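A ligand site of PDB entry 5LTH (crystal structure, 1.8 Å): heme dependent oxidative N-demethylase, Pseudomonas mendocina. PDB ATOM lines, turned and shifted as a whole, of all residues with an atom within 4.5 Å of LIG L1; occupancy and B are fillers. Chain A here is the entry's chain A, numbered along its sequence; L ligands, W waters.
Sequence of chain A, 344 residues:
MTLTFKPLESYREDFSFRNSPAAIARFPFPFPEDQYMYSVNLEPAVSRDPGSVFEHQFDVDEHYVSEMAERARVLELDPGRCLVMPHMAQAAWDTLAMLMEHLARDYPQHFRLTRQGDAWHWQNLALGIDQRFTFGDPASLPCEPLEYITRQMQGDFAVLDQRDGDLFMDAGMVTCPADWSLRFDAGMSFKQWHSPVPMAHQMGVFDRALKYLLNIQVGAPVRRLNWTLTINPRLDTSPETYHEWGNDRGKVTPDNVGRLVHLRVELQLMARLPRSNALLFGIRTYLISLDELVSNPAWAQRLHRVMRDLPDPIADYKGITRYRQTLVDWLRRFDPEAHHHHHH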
ATOM      1  N   TYR A  38      12.137  15.654   1.325  1.00  0.00           N
ATOM      2  CA  TYR A  38      11.640  14.493   0.661  1.00  0.00           C
ATOM      3  C   TYR A  38      12.484  14.157  -0.591  1.00  0.00           C
ATOM      4  O   TYR A  38      13.027  15.080  -1.264  1.00  0.00           O
ATOM      5  CB  TYR A  38      10.189  14.719   0.159  1.00  0.00           C
ATOM      6  CG  TYR A  38       9.083  15.001   1.207  1.00  0.00           C
ATOM      7  CD1 TYR A  38       9.032  14.224   2.368  1.00  0.00           C
ATOM      8  CD2 TYR A  38       8.125  15.977   1.004  1.00  0.00           C
ATOM      9  CE1 TYR A  38       8.027  14.387   3.270  1.00  0.00           C
ATOM     10  CE2 TYR A  38       7.100  16.198   1.887  1.00  0.00           C
ATOM     11  CZ  TYR A  38       7.075  15.322   3.083  1.00  0.00           C
ATOM     12  OH  TYR A  38       5.990  15.542   3.910  1.00  0.00           O
ATOM     13  N   SER A  39      12.598  12.863  -0.920  1.00  0.00           N
ATOM     14  CA  SER A  39      13.283  12.386  -2.084  1.00  0.00           C
ATOM     15  C   SER A  39      12.810  10.948  -2.395  1.00  0.00           C
ATOM     16  O   SER A  39      12.199  10.335  -1.511  1.00  0.00           O
ATOM     17  CB  SER A  39      14.759  12.389  -1.805  1.00  0.00           C
ATOM     18  OG  SER A  39      15.237  11.395  -0.909  1.00  0.00           O
ATOM     19  N   VAL A  40      13.286  10.371  -3.486  1.00  0.00           N
ATOM     20  CA  VAL A  40      13.090   8.940  -3.762  1.00  0.00           C
ATOM     21  C   VAL A  40      14.250   8.214  -3.114  1.00  0.00           C
ATOM     22  O   VAL A  40      15.334   7.987  -3.695  1.00  0.00           O
ATOM     23  CB  VAL A  40      12.890   8.641  -5.278  1.00  0.00           C
ATOM     24  CG1 VAL A  40      12.542   7.143  -5.443  1.00  0.00           C
ATOM     25  CG2 VAL A  40      11.762   9.442  -5.836  1.00  0.00           C
ATOM     26  N   ASN A  41      14.091   7.918  -1.823  1.00  0.00           N
ATOM     27  CA  ASN A  41      15.164   7.387  -1.026  1.00  0.00           C
ATOM     28  C   ASN A  41      15.162   5.828  -0.961  1.00  0.00           C
ATOM     29  O   ASN A  41      15.350   5.254   0.117  1.00  0.00           O
ATOM     30  CB  ASN A  41      15.179   8.006   0.416  1.00  0.00           C
ATOM     31  CG  ASN A  41      13.868   7.758   1.160  1.00  0.00           C
ATOM     32  OD1 ASN A  41      12.813   7.661   0.544  1.00  0.00           O
ATOM     33  ND2 ASN A  41      13.939   7.792   2.445  1.00  0.00           N
ATOM     34  N   LEU A  42      14.936   5.246  -2.086  1.00  0.00           N
ATOM     35  CA  LEU A  42      14.780   3.785  -2.210  1.00  0.00           C
ATOM     36  C   LEU A  42      16.129   3.170  -2.322  1.00  0.00           C
ATOM     37  O   LEU A  42      17.034   3.731  -2.987  1.00  0.00           O
ATOM     38  CB  LEU A  42      13.930   3.444  -3.328  1.00  0.00           C
ATOM     39  CG  LEU A  42      12.452   3.785  -3.199  1.00  0.00           C
ATOM     40  CD1 LEU A  42      11.852   3.628  -4.544  1.00  0.00           C
ATOM     41  CD2 LEU A  42      11.756   2.911  -2.163  1.00  0.00           C
ATOM     42  N   ALA A 158       0.373  -3.138   3.674  1.00  0.00           N
ATOM     43  CA  ALA A 158      -0.559  -2.956   2.626  1.00  0.00           C
ATOM     44  C   ALA A 158      -0.227  -3.911   1.503  1.00  0.00           C
ATOM     45  O   ALA A 158       0.964  -4.282   1.323  1.00  0.00           O
ATOM     46  CB  ALA A 158      -0.592  -1.539   2.068  1.00  0.00           C
ATOM     47  N   LEU A 160      -0.855  -4.335  -2.536  1.00  0.00           N
ATOM     48  CA  LEU A 160      -1.308  -3.551  -3.608  1.00  0.00           C
ATOM     49  C   LEU A 160      -1.514  -4.416  -4.910  1.00  0.00           C
ATOM     50  O   LEU A 160      -0.600  -5.209  -5.263  1.00  0.00           O
ATOM     51  CB  LEU A 160      -0.241  -2.483  -3.950  1.00  0.00           C
ATOM     52  CG  LEU A 160       0.192  -1.438  -2.903  1.00  0.00           C
ATOM     53  CD1 LEU A 160      -1.034  -0.866  -2.301  1.00  0.00           C
ATOM     54  CD2 LEU A 160       1.136  -1.978  -1.858  1.00  0.00           C
ATOM     55  N   MET A 169      -4.660   0.138  -3.519  1.00  0.00           N
ATOM     56  CA  MET A 169      -4.675  -0.324  -2.143  1.00  0.00           C
ATOM     57  C   MET A 169      -5.871  -1.207  -1.807  1.00  0.00           C
ATOM     58  O   MET A 169      -6.910  -0.778  -1.293  1.00  0.00           O
ATOM     59  CB  MET A 169      -4.546   0.842  -1.141  1.00  0.00           C
ATOM     60  CG  MET A 169      -4.054   0.369   0.220  1.00  0.00           C
ATOM     61  SD  MET A 169      -4.096   1.657   1.508  1.00  0.00           S
ATOM     62  CE  MET A 169      -2.854   2.806   0.959  1.00  0.00           C
ATOM     63  N   ASP A 179      -1.442   8.445  11.182  1.00  0.00           N
ATOM     64  CA  ASP A 179      -2.545   9.325  10.931  1.00  0.00           C
ATOM     65  C   ASP A 179      -3.091   9.219   9.503  1.00  0.00           C
ATOM     66  O   ASP A 179      -3.323  10.184   8.745  1.00  0.00           O
ATOM     67  CB  ASP A 179      -2.136  10.797  11.252  1.00  0.00           C
ATOM     68  CG  ASP A 179      -3.368  11.694  11.305  1.00  0.00           C
ATOM     69  OD1 ASP A 179      -4.518  11.171  11.543  1.00  0.00           O
ATOM     70  OD2 ASP A 179      -3.226  12.910  11.187  1.00  0.00           O
ATOM     71  N   TRP A 180      -3.501   7.958   9.116  1.00  0.00           N
ATOM     72  CA  TRP A 180      -4.252   7.709   7.941  1.00  0.00           C
ATOM     73  C   TRP A 180      -5.022   6.360   8.224  1.00  0.00           C
ATOM     74  O   TRP A 180      -4.791   5.756   9.288  1.00  0.00           O
ATOM     75  CB  TRP A 180      -3.368   7.548   6.700  1.00  0.00           C
ATOM     76  CG  TRP A 180      -2.321   6.425   6.667  1.00  0.00           C
ATOM     77  CD1 TRP A 180      -1.116   6.391   7.354  1.00  0.00           C
ATOM     78  CD2 TRP A 180      -2.484   5.115   6.116  1.00  0.00           C
ATOM     79  NE1 TRP A 180      -0.505   5.175   7.164  1.00  0.00           N
ATOM     80  CE2 TRP A 180      -1.324   4.381   6.420  1.00  0.00           C
ATOM     81  CE3 TRP A 180      -3.420   4.542   5.331  1.00  0.00           C
ATOM     82  CZ2 TRP A 180      -1.104   3.062   5.958  1.00  0.00           C
ATOM     83  CZ3 TRP A 180      -3.253   3.280   4.895  1.00  0.00           C
ATOM     84  CH2 TRP A 180      -2.052   2.579   5.172  1.00  0.00           C
ATOM     85  N   ASP A 185      -8.692   4.704   2.451  1.00  0.00           N
ATOM     86  CA  ASP A 185      -7.840   4.633   1.286  1.00  0.00           C
ATOM     87  C   ASP A 185      -8.087   3.387   0.402  1.00  0.00           C
ATOM     88  O   ASP A 185      -7.543   3.275  -0.727  1.00  0.00           O
ATOM     89  CB  ASP A 185      -6.360   4.745   1.653  1.00  0.00           C
ATOM     90  CG  ASP A 185      -5.951   6.101   2.156  1.00  0.00           C
ATOM     91  OD1 ASP A 185      -6.769   6.999   2.410  1.00  0.00           O
ATOM     92  OD2 ASP A 185      -4.735   6.276   2.261  1.00  0.00           O
ATOM     93  N   PHE A 190      -2.048   4.927  -6.343  1.00  0.00           N
ATOM     94  CA  PHE A 190      -0.785   5.441  -5.727  1.00  0.00           C
ATOM     95  C   PHE A 190      -0.773   6.986  -5.543  1.00  0.00           C
ATOM     96  O   PHE A 190      -0.529   7.492  -4.455  1.00  0.00           O
ATOM     97  CB  PHE A 190       0.370   4.924  -6.473  1.00  0.00           C
ATOM     98  CG  PHE A 190       1.733   5.238  -5.890  1.00  0.00           C
ATOM     99  CD1 PHE A 190       2.319   4.358  -5.027  1.00  0.00           C
ATOM    100  CD2 PHE A 190       2.527   6.411  -6.221  1.00  0.00           C
ATOM    101  CE1 PHE A 190       3.516   4.568  -4.445  1.00  0.00           C
ATOM    102  CE2 PHE A 190       3.793   6.556  -5.642  1.00  0.00           C
ATOM    103  CZ  PHE A 190       4.257   5.700  -4.701  1.00  0.00           C
ATOM    104  N   TRP A 193      -3.881   8.235  -3.103  1.00  0.00           N
ATOM    105  CA  TRP A 193      -3.790   8.135  -1.613  1.00  0.00           C
ATOM    106  C   TRP A 193      -2.695   9.077  -1.074  1.00  0.00           C
ATOM    107  O   TRP A 193      -2.680   9.425   0.094  1.00  0.00           O
ATOM    108  CB  TRP A 193      -3.625   6.676  -1.153  1.00  0.00           C
ATOM    109  CG  TRP A 193      -2.327   5.998  -1.296  1.00  0.00           C
ATOM    110  CD1 TRP A 193      -1.143   6.394  -0.755  1.00  0.00           C
ATOM    111  CD2 TRP A 193      -2.002   4.843  -2.095  1.00  0.00           C
ATOM    112  NE1 TRP A 193      -0.126   5.544  -1.122  1.00  0.00           N
ATOM    113  CE2 TRP A 193      -0.640   4.598  -1.958  1.00  0.00           C
ATOM    114  CE3 TRP A 193      -2.783   3.960  -2.904  1.00  0.00           C
ATOM    115  CZ2 TRP A 193       0.001   3.499  -2.520  1.00  0.00           C
ATOM    116  CZ3 TRP A 193      -2.106   2.935  -3.509  1.00  0.00           C
ATOM    117  CH2 TRP A 193      -0.728   2.746  -3.362  1.00  0.00           C
ATOM    118  N   HIS A 194      -1.750   9.528  -1.950  1.00  0.00           N
ATOM    119  CA  HIS A 194      -0.700  10.447  -1.539  1.00  0.00           C
ATOM    120  C   HIS A 194      -1.099  11.876  -1.696  1.00  0.00           C
ATOM    121  O   HIS A 194      -0.257  12.771  -1.440  1.00  0.00           O
ATOM    122  CB  HIS A 194       0.564  10.199  -2.338  1.00  0.00           C
ATOM    123  CG  HIS A 194       1.373   9.043  -1.893  1.00  0.00           C
ATOM    124  ND1 HIS A 194       1.645   7.934  -2.657  1.00  0.00           N
ATOM    125  CD2 HIS A 194       1.978   8.829  -0.710  1.00  0.00           C
ATOM    126  CE1 HIS A 194       2.486   7.147  -2.032  1.00  0.00           C
ATOM    127  NE2 HIS A 194       2.692   7.655  -0.807  1.00  0.00           N
ATOM    128  N   PRO A 196      -2.707  14.165   0.045  1.00  0.00           N
ATOM    129  CA  PRO A 196      -2.445  15.154   1.107  1.00  0.00           C
ATOM    130  C   PRO A 196      -1.012  15.615   1.332  1.00  0.00           C
ATOM    131  O   PRO A 196      -0.817  16.597   2.098  1.00  0.00           O
ATOM    132  CB  PRO A 196      -2.925  14.403   2.376  1.00  0.00           C
ATOM    133  CG  PRO A 196      -3.730  13.212   1.894  1.00  0.00           C
ATOM    134  CD  PRO A 196      -3.168  12.848   0.571  1.00  0.00           C
ATOM    135  N   VAL A 197      -0.025  14.960   0.745  1.00  0.00           N
ATOM    136  CA  VAL A 197       1.382  15.200   1.070  1.00  0.00           C
ATOM    137  C   VAL A 197       1.831  16.497   0.331  1.00  0.00           C
ATOM    138  O   VAL A 197       1.645  16.608  -0.932  1.00  0.00           O
ATOM    139  CB  VAL A 197       2.250  14.049   0.618  1.00  0.00           C
ATOM    140  CG1 VAL A 197       3.714  14.314   0.949  1.00  0.00           C
ATOM    141  CG2 VAL A 197       1.832  12.752   1.323  1.00  0.00           C
ATOM    142  N   VAL A 205       8.412  13.308  -6.976  1.00  0.00           N
ATOM    143  CA  VAL A 205       8.874  12.251  -6.124  1.00  0.00           C
ATOM    144  C   VAL A 205       7.914  11.056  -6.384  1.00  0.00           C
ATOM    145  O   VAL A 205       8.360   9.884  -6.473  1.00  0.00           O
ATOM    146  CB  VAL A 205       8.866  12.655  -4.643  1.00  0.00           C
ATOM    147  CG1 VAL A 205       8.952  11.518  -3.745  1.00  0.00           C
ATOM    148  CG2 VAL A 205      10.124  13.490  -4.338  1.00  0.00           C
ATOM    149  N   PHE A 206       6.663  11.396  -6.430  1.00  0.00           N
ATOM    150  CA  PHE A 206       5.585  10.305  -6.539  1.00  0.00           C
ATOM    151  C   PHE A 206       5.549   9.699  -7.953  1.00  0.00           C
ATOM    152  O   PHE A 206       5.481   8.480  -8.108  1.00  0.00           O
ATOM    153  CB  PHE A 206       4.253  10.723  -6.076  1.00  0.00           C
ATOM    154  CG  PHE A 206       4.208  10.964  -4.625  1.00  0.00           C
ATOM    155  CD1 PHE A 206       4.506   9.954  -3.722  1.00  0.00           C
ATOM    156  CD2 PHE A 206       3.791  12.167  -4.121  1.00  0.00           C
ATOM    157  CE1 PHE A 206       4.505  10.232  -2.350  1.00  0.00           C
ATOM    158  CE2 PHE A 206       3.722  12.428  -2.756  1.00  0.00           C
ATOM    159  CZ  PHE A 206       4.105  11.471  -1.858  1.00  0.00           C
ATOM    160  N   ALA A 209       8.757   7.477  -7.916  1.00  0.00           N
ATOM    161  CA  ALA A 209       8.607   6.370  -6.998  1.00  0.00           C
ATOM    162  C   ALA A 209       7.689   5.283  -7.628  1.00  0.00           C
ATOM    163  O   ALA A 209       8.015   4.110  -7.549  1.00  0.00           O
ATOM    164  CB  ALA A 209       8.002   6.908  -5.673  1.00  0.00           C
ATOM    165  N   LEU A 213       8.640   1.311  -8.305  1.00  0.00           N
ATOM    166  CA  LEU A 213       7.796   0.257  -7.618  1.00  0.00           C
ATOM    167  C   LEU A 213       7.161  -0.704  -8.703  1.00  0.00           C
ATOM    168  O   LEU A 213       7.147  -1.945  -8.485  1.00  0.00           O
ATOM    169  CB  LEU A 213       6.726   0.886  -6.661  1.00  0.00           C
ATOM    170  CG  LEU A 213       7.268   0.992  -5.254  1.00  0.00           C
ATOM    171  CD1 LEU A 213       8.556   1.805  -5.121  1.00  0.00           C
ATOM    172  CD2 LEU A 213       6.147   1.536  -4.465  1.00  0.00           C
ATOM    173  N   ARG A 224      12.923   1.744   2.055  1.00  0.00           N
ATOM    174  CA  ARG A 224      13.213   3.111   2.396  1.00  0.00           C
ATOM    175  C   ARG A 224      12.788   3.396   3.876  1.00  0.00           C
ATOM    176  O   ARG A 224      12.058   2.607   4.449  1.00  0.00           O
ATOM    177  CB  ARG A 224      12.484   4.047   1.537  1.00  0.00           C
ATOM    178  CG  ARG A 224      10.928   4.099   1.660  1.00  0.00           C
ATOM    179  CD  ARG A 224      10.181   5.163   0.834  1.00  0.00           C
ATOM    180  NE  ARG A 224      10.313   6.534   1.283  1.00  0.00           N
ATOM    181  CZ  ARG A 224       9.431   7.181   2.080  1.00  0.00           C
ATOM    182  NH1 ARG A 224       8.314   6.579   2.544  1.00  0.00           N
ATOM    183  NH2 ARG A 224       9.610   8.437   2.422  1.00  0.00           N
ATOM    184  N   ASN A 226      10.747   6.237   6.332  1.00  0.00           N
ATOM    185  CA  ASN A 226       9.929   7.416   6.571  1.00  0.00           C
ATOM    186  C   ASN A 226       9.983   7.698   8.092  1.00  0.00           C
ATOM    187  O   ASN A 226      10.458   6.854   8.903  1.00  0.00           O
ATOM    188  CB  ASN A 226       8.448   7.235   6.154  1.00  0.00           C
ATOM    189  CG  ASN A 226       7.791   8.570   5.934  1.00  0.00           C
ATOM    190  OD1 ASN A 226       8.154   9.299   4.997  1.00  0.00           O
ATOM    191  ND2 ASN A 226       6.873   8.954   6.823  1.00  0.00           N
ATOM    192  N   TRP A 227       9.639   8.918   8.471  1.00  0.00           N
ATOM    193  CA  TRP A 227       9.641   9.297   9.899  1.00  0.00           C
ATOM    194  C   TRP A 227       8.548  10.298  10.174  1.00  0.00           C
ATOM    195  O   TRP A 227       8.014  10.998   9.279  1.00  0.00           O
ATOM    196  CB  TRP A 227      11.010   9.866  10.268  1.00  0.00           C
ATOM    197  CG  TRP A 227      11.212  11.219   9.726  1.00  0.00           C
ATOM    198  CD1 TRP A 227      11.624  11.497   8.461  1.00  0.00           C
ATOM    199  CD2 TRP A 227      10.986  12.505  10.359  1.00  0.00           C
ATOM    200  NE1 TRP A 227      11.692  12.852   8.292  1.00  0.00           N
ATOM    201  CE2 TRP A 227      11.281  13.497   9.398  1.00  0.00           C
ATOM    202  CE3 TRP A 227      10.520  12.928  11.629  1.00  0.00           C
ATOM    203  CZ2 TRP A 227      11.099  14.841   9.655  1.00  0.00           C
ATOM    204  CZ3 TRP A 227      10.300  14.284  11.858  1.00  0.00           C
ATOM    205  CH2 TRP A 227      10.681  15.226  10.901  1.00  0.00           C
ATOM    206  N   MET A 270       9.199  -3.082   0.154  1.00  0.00           N
ATOM    207  CA  MET A 270       8.399  -3.325  -1.001  1.00  0.00           C
ATOM    208  C   MET A 270       8.959  -4.577  -1.757  1.00  0.00           C
ATOM    209  O   MET A 270      10.132  -4.632  -2.231  1.00  0.00           O
ATOM    210  CB  MET A 270       8.392  -2.132  -1.965  1.00  0.00           C
ATOM    211  CG  MET A 270       7.733  -0.894  -1.380  1.00  0.00           C
ATOM    212  SD  MET A 270       8.666   0.668  -1.430  1.00  0.00           S
ATOM    213  CE  MET A 270       9.809   0.491  -0.104  1.00  0.00           C
ATOM    214  N   PHE A 281       3.729  -4.137   0.798  1.00  0.00           N
ATOM    215  CA  PHE A 281       4.320  -2.940   1.437  1.00  0.00           C
ATOM    216  C   PHE A 281       4.292  -3.103   2.953  1.00  0.00           C
ATOM    217  O   PHE A 281       3.210  -3.104   3.535  1.00  0.00           O
ATOM    218  CB  PHE A 281       3.499  -1.697   1.042  1.00  0.00           C
ATOM    219  CG  PHE A 281       4.045  -0.348   1.555  1.00  0.00           C
ATOM    220  CD1 PHE A 281       5.292   0.118   1.167  1.00  0.00           C
ATOM    221  CD2 PHE A 281       3.252   0.447   2.362  1.00  0.00           C
ATOM    222  CE1 PHE A 281       5.708   1.401   1.547  1.00  0.00           C
ATOM    223  CE2 PHE A 281       3.676   1.723   2.723  1.00  0.00           C
ATOM    224  CZ  PHE A 281       4.893   2.159   2.354  1.00  0.00           C
ATOM    225  N   TYR A 317       2.238  19.104   7.929  1.00  0.00           N
ATOM    226  CA  TYR A 317       1.715  17.818   7.471  1.00  0.00           C
ATOM    227  C   TYR A 317       1.975  16.746   8.532  1.00  0.00           C
ATOM    228  O   TYR A 317       1.024  15.879   8.814  1.00  0.00           O
ATOM    229  CB  TYR A 317       2.323  17.491   6.101  1.00  0.00           C
ATOM    230  CG  TYR A 317       2.009  15.982   5.777  1.00  0.00           C
ATOM    231  CD1 TYR A 317       0.773  15.652   5.295  1.00  0.00           C
ATOM    232  CD2 TYR A 317       2.920  15.008   6.074  1.00  0.00           C
ATOM    233  CE1 TYR A 317       0.414  14.322   5.056  1.00  0.00           C
ATOM    234  CE2 TYR A 317       2.562  13.653   5.894  1.00  0.00           C
ATOM    235  CZ  TYR A 317       1.311  13.340   5.411  1.00  0.00           C
ATOM    236  OH  TYR A 317       0.984  11.982   5.238  1.00  0.00           O
ATOM    237  N   LYS A 318       3.160  16.685   9.086  1.00  0.00           N
ATOM    238  CA  LYS A 318       3.630  15.715  10.065  1.00  0.00           C
ATOM    239  C   LYS A 318       2.931  15.853  11.430  1.00  0.00           C
ATOM    240  O   LYS A 318       3.015  14.960  12.235  1.00  0.00           O
ATOM    241  CB  LYS A 318       5.139  15.593  10.180  1.00  0.00           C
ATOM    242  CG  LYS A 318       5.888  15.065   8.942  1.00  0.00           C
ATOM    243  CD  LYS A 318       7.353  15.145   9.115  1.00  0.00           C
ATOM    244  CE  LYS A 318       8.131  14.688   7.862  1.00  0.00           C
ATOM    245  NZ  LYS A 318       8.129  13.186   7.717  1.00  0.00           N
HETATM  246  C1  LIG L   1       2.688   9.312   2.931  1.00  0.00           C
HETATM  247  C2  LIG L   1       1.206   4.912   1.527  1.00  0.00           C
HETATM  248  C3  LIG L   1       5.276   4.280  -1.132  1.00  0.00           C
HETATM  249  C4  LIG L   1       6.618   8.816   0.040  1.00  0.00           C
HETATM  250  C5  LIG L   1       1.940   8.186   2.772  1.00  0.00           C
HETATM  251  C6  LIG L   1       0.611   7.987   3.342  1.00  0.00           C
HETATM  252  C7  LIG L   1       0.262   6.745   2.910  1.00  0.00           C
HETATM  253  C8  LIG L   1       1.267   6.194   2.082  1.00  0.00           C
HETATM  254  C9  LIG L   1      -1.067   6.082   3.149  1.00  0.00           C
HETATM  255  C10 LIG L   1      -0.085   8.946   4.234  1.00  0.00           C
HETATM  256  C11 LIG L   1      -0.847   9.954   3.397  1.00  0.00           C
HETATM  257  C12 LIG L   1      -1.874  10.645   4.218  1.00  0.00           C
HETATM  258  O1  LIG L   1      -3.085  10.360   4.234  1.00  0.00           O
HETATM  259  O2  LIG L   1      -1.532  11.649   4.928  1.00  0.00           O
HETATM  260  C13 LIG L   1       2.212   4.347   0.749  1.00  0.00           C
HETATM  261  C14 LIG L   1       2.156   3.026   0.169  1.00  0.00           C
HETATM  262  C15 LIG L   1       3.291   2.858  -0.619  1.00  0.00           C
HETATM  263  C16 LIG L   1       4.099   4.115  -0.480  1.00  0.00           C
HETATM  264  C17 LIG L   1       1.030   2.034   0.383  1.00  0.00           C
HETATM  265  C18 LIG L   1       3.752   1.751  -1.452  1.00  0.00           C
HETATM  266  C19 LIG L   1       2.869   1.050  -2.127  1.00  0.00           C
HETATM  267  C20 LIG L   1       6.005   5.429  -1.077  1.00  0.00           C
HETATM  268  C21 LIG L   1       7.306   5.589  -1.628  1.00  0.00           C
HETATM  269  C22 LIG L   1       7.669   6.927  -1.335  1.00  0.00           C
HETATM  270  C23 LIG L   1       6.593   7.522  -0.519  1.00  0.00           C
HETATM  271  C24 LIG L   1       8.030   4.634  -2.472  1.00  0.00           C
HETATM  272  C25 LIG L   1       8.955   7.441  -1.833  1.00  0.00           C
HETATM  273  C26 LIG L   1       9.313   8.542  -1.583  1.00  0.00           C
HETATM  274  C27 LIG L   1       5.667   9.253   0.928  1.00  0.00           C
HETATM  275  C28 LIG L   1       5.783  10.553   1.581  1.00  0.00           C
HETATM  276  C29 LIG L   1       4.730  10.715   2.461  1.00  0.00           C
HETATM  277  C30 LIG L   1       3.930   9.451   2.302  1.00  0.00           C
HETATM  278  C31 LIG L   1       6.999  11.494   1.393  1.00  0.00           C
HETATM  279  C32 LIG L   1       4.502  11.778   3.458  1.00  0.00           C
HETATM  280  C33 LIG L   1       5.106  11.255   4.766  1.00  0.00           C
HETATM  281  C34 LIG L   1       5.585  12.198   5.811  1.00  0.00           C
HETATM  282  O3  LIG L   1       5.875  13.408   5.583  1.00  0.00           O
HETATM  283  O4  LIG L   1       5.826  11.735   6.989  1.00  0.00           O
HETATM  284  N1  LIG L   1       2.318   7.084   2.003  1.00  0.00           N
HETATM  285  N2  LIG L   1       3.339   4.941   0.297  1.00  0.00           N
HETATM  286  N3  LIG L   1       5.579   6.585  -0.375  1.00  0.00           N
HETATM  287  N4  LIG L   1       4.495   8.673   1.298  1.00  0.00           N
HETATM  288 FE1  LIG L   1       3.903   6.856   0.785  1.00  0.00          FE
HETATM  289  N1  LG2 L   2       3.852   6.225   5.685  1.00  0.00           N
HETATM  290  C1  LG2 L   2       2.872   5.158   5.147  1.00  0.00           C
HETATM  291  C2  LG2 L   2       3.128   7.366   6.242  1.00  0.00           C
HETATM  292  O   HOH W   1      -4.112   8.834   2.350  1.00  0.00           O
HETATM  293  O   HOH W   2      -3.534  13.641   5.717  1.00  0.00           O
HETATM  294  O   HOH W   3       5.075   6.216   2.928  1.00  0.00           O
HETATM  295  O   HOH W   4      -5.280  10.660   5.554  1.00  0.00           O
HETATM  296  O   HOH W   5       4.133  10.344   8.601  1.00  0.00           O
HETATM  297  O   HOH W   6      -1.128  11.915   7.846  1.00  0.00           O
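An oxygen (O4) of LIG L1 sits close to the backbone carbonyl oxygen of Trp 227 (3.3 Å). Residues that only touch LIG L1: Trp 193 (3.0 Å), Phe 281 (3.2 Å), Ser 39 (3.4 Å), Trp 180 (3.4 Å), Phe 206 (3.5 Å), Leu 160 (3.5 Å), Arg 224 (3.5 Å), Val 197 (3.6 Å), Val 205 (3.7 Å), Pro 196 (3.7 Å), Phe 190 (3.8 Å), Asp 185 (3.8 Å), Leu 213 (3.9 Å) and Ala 209 (3.9 Å). Hydrophobic or aromatic side chains within 4 Å of LIG L1: Tyr 38, Leu 160, Trp 180, Phe 190, Trp 193, His 194, Pro 196, Val 197, Val 205, Phe 206, Ala 209, Leu 213, Phe 281 and Tyr 317. 20 residues have an atom within 4 Å of LIG L1: Tyr 38, Ser 39, Leu 160, Trp 180, Asp 185, Phe 190, Trp 193, His 194, Pro 196, Val 197, Val 205, Phe 206, Ala 209, Leu 213, Arg 224, Asn 226, Trp 227, Phe 281, Tyr 317 and Lys 318.
FE1 of LIG L1 is bound by NE2 of His 194, 2.2 Å away. OH of Tyr 317 sits at hydrogen-bond distance from O2 of LIG L1, at 2.6 Å. The side-chain hydroxyl (OH) of Tyr 38 is in hydrogen-bond range of an oxygen (O3) of LIG L1 (2.7 Å). An oxygen (O4) of LIG L1 lies within salt-bridge range of the side-chain amino group of Lys 318, at 2.8 Å. The side-chain amide nitrogen (ND2) of Asn 226 is in hydrogen-bond range of an oxygen (O4) of LIG L1.
Water W3 lies within hydrogen-bond range of N1 of LG2 L2 (3.0 Å) and NH1 of Arg 224 (3.3 Å). Water W1 lies within hydrogen-bond range of O1 of LIG L1, OD2 of Asp 185 and O of Trp 193. Water W6 lies within hydrogen-bond range of the backbone carbonyl oxygen (O) of Asp 179 (2.9 Å), an oxygen (O2) of LIG L1 (3.0 Å) and the side-chain hydroxyl (OH) of Tyr 317 (3.4 Å).
The indole nitrogen of Trp 193 lies close to a ring nitrogen (ND1) of His 194 (3.3 Å). ND1 of His 194 is in hydrogen-bond range of O of Phe 190 (2.9 Å). NZ of Lys 318 sits at hydrogen-bond distance from O of Trp 227 (2.7 Å). NH2 of Arg 224 sits at hydrogen-bond distance from OD1 of Asn 226, at 3.1 Å. The backbone NH of Phe 281 lies within hydrogen-bond range of the backbone carbonyl oxygen of Ala 158, at 2.8 Å. The backbone carbonyl oxygen of Ser 39 sits close to the side-chain amide oxygen of Asn 41. NE of Arg 224 sits at hydrogen-bond distance from OD1 of Asn 41 (2.8 Å).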
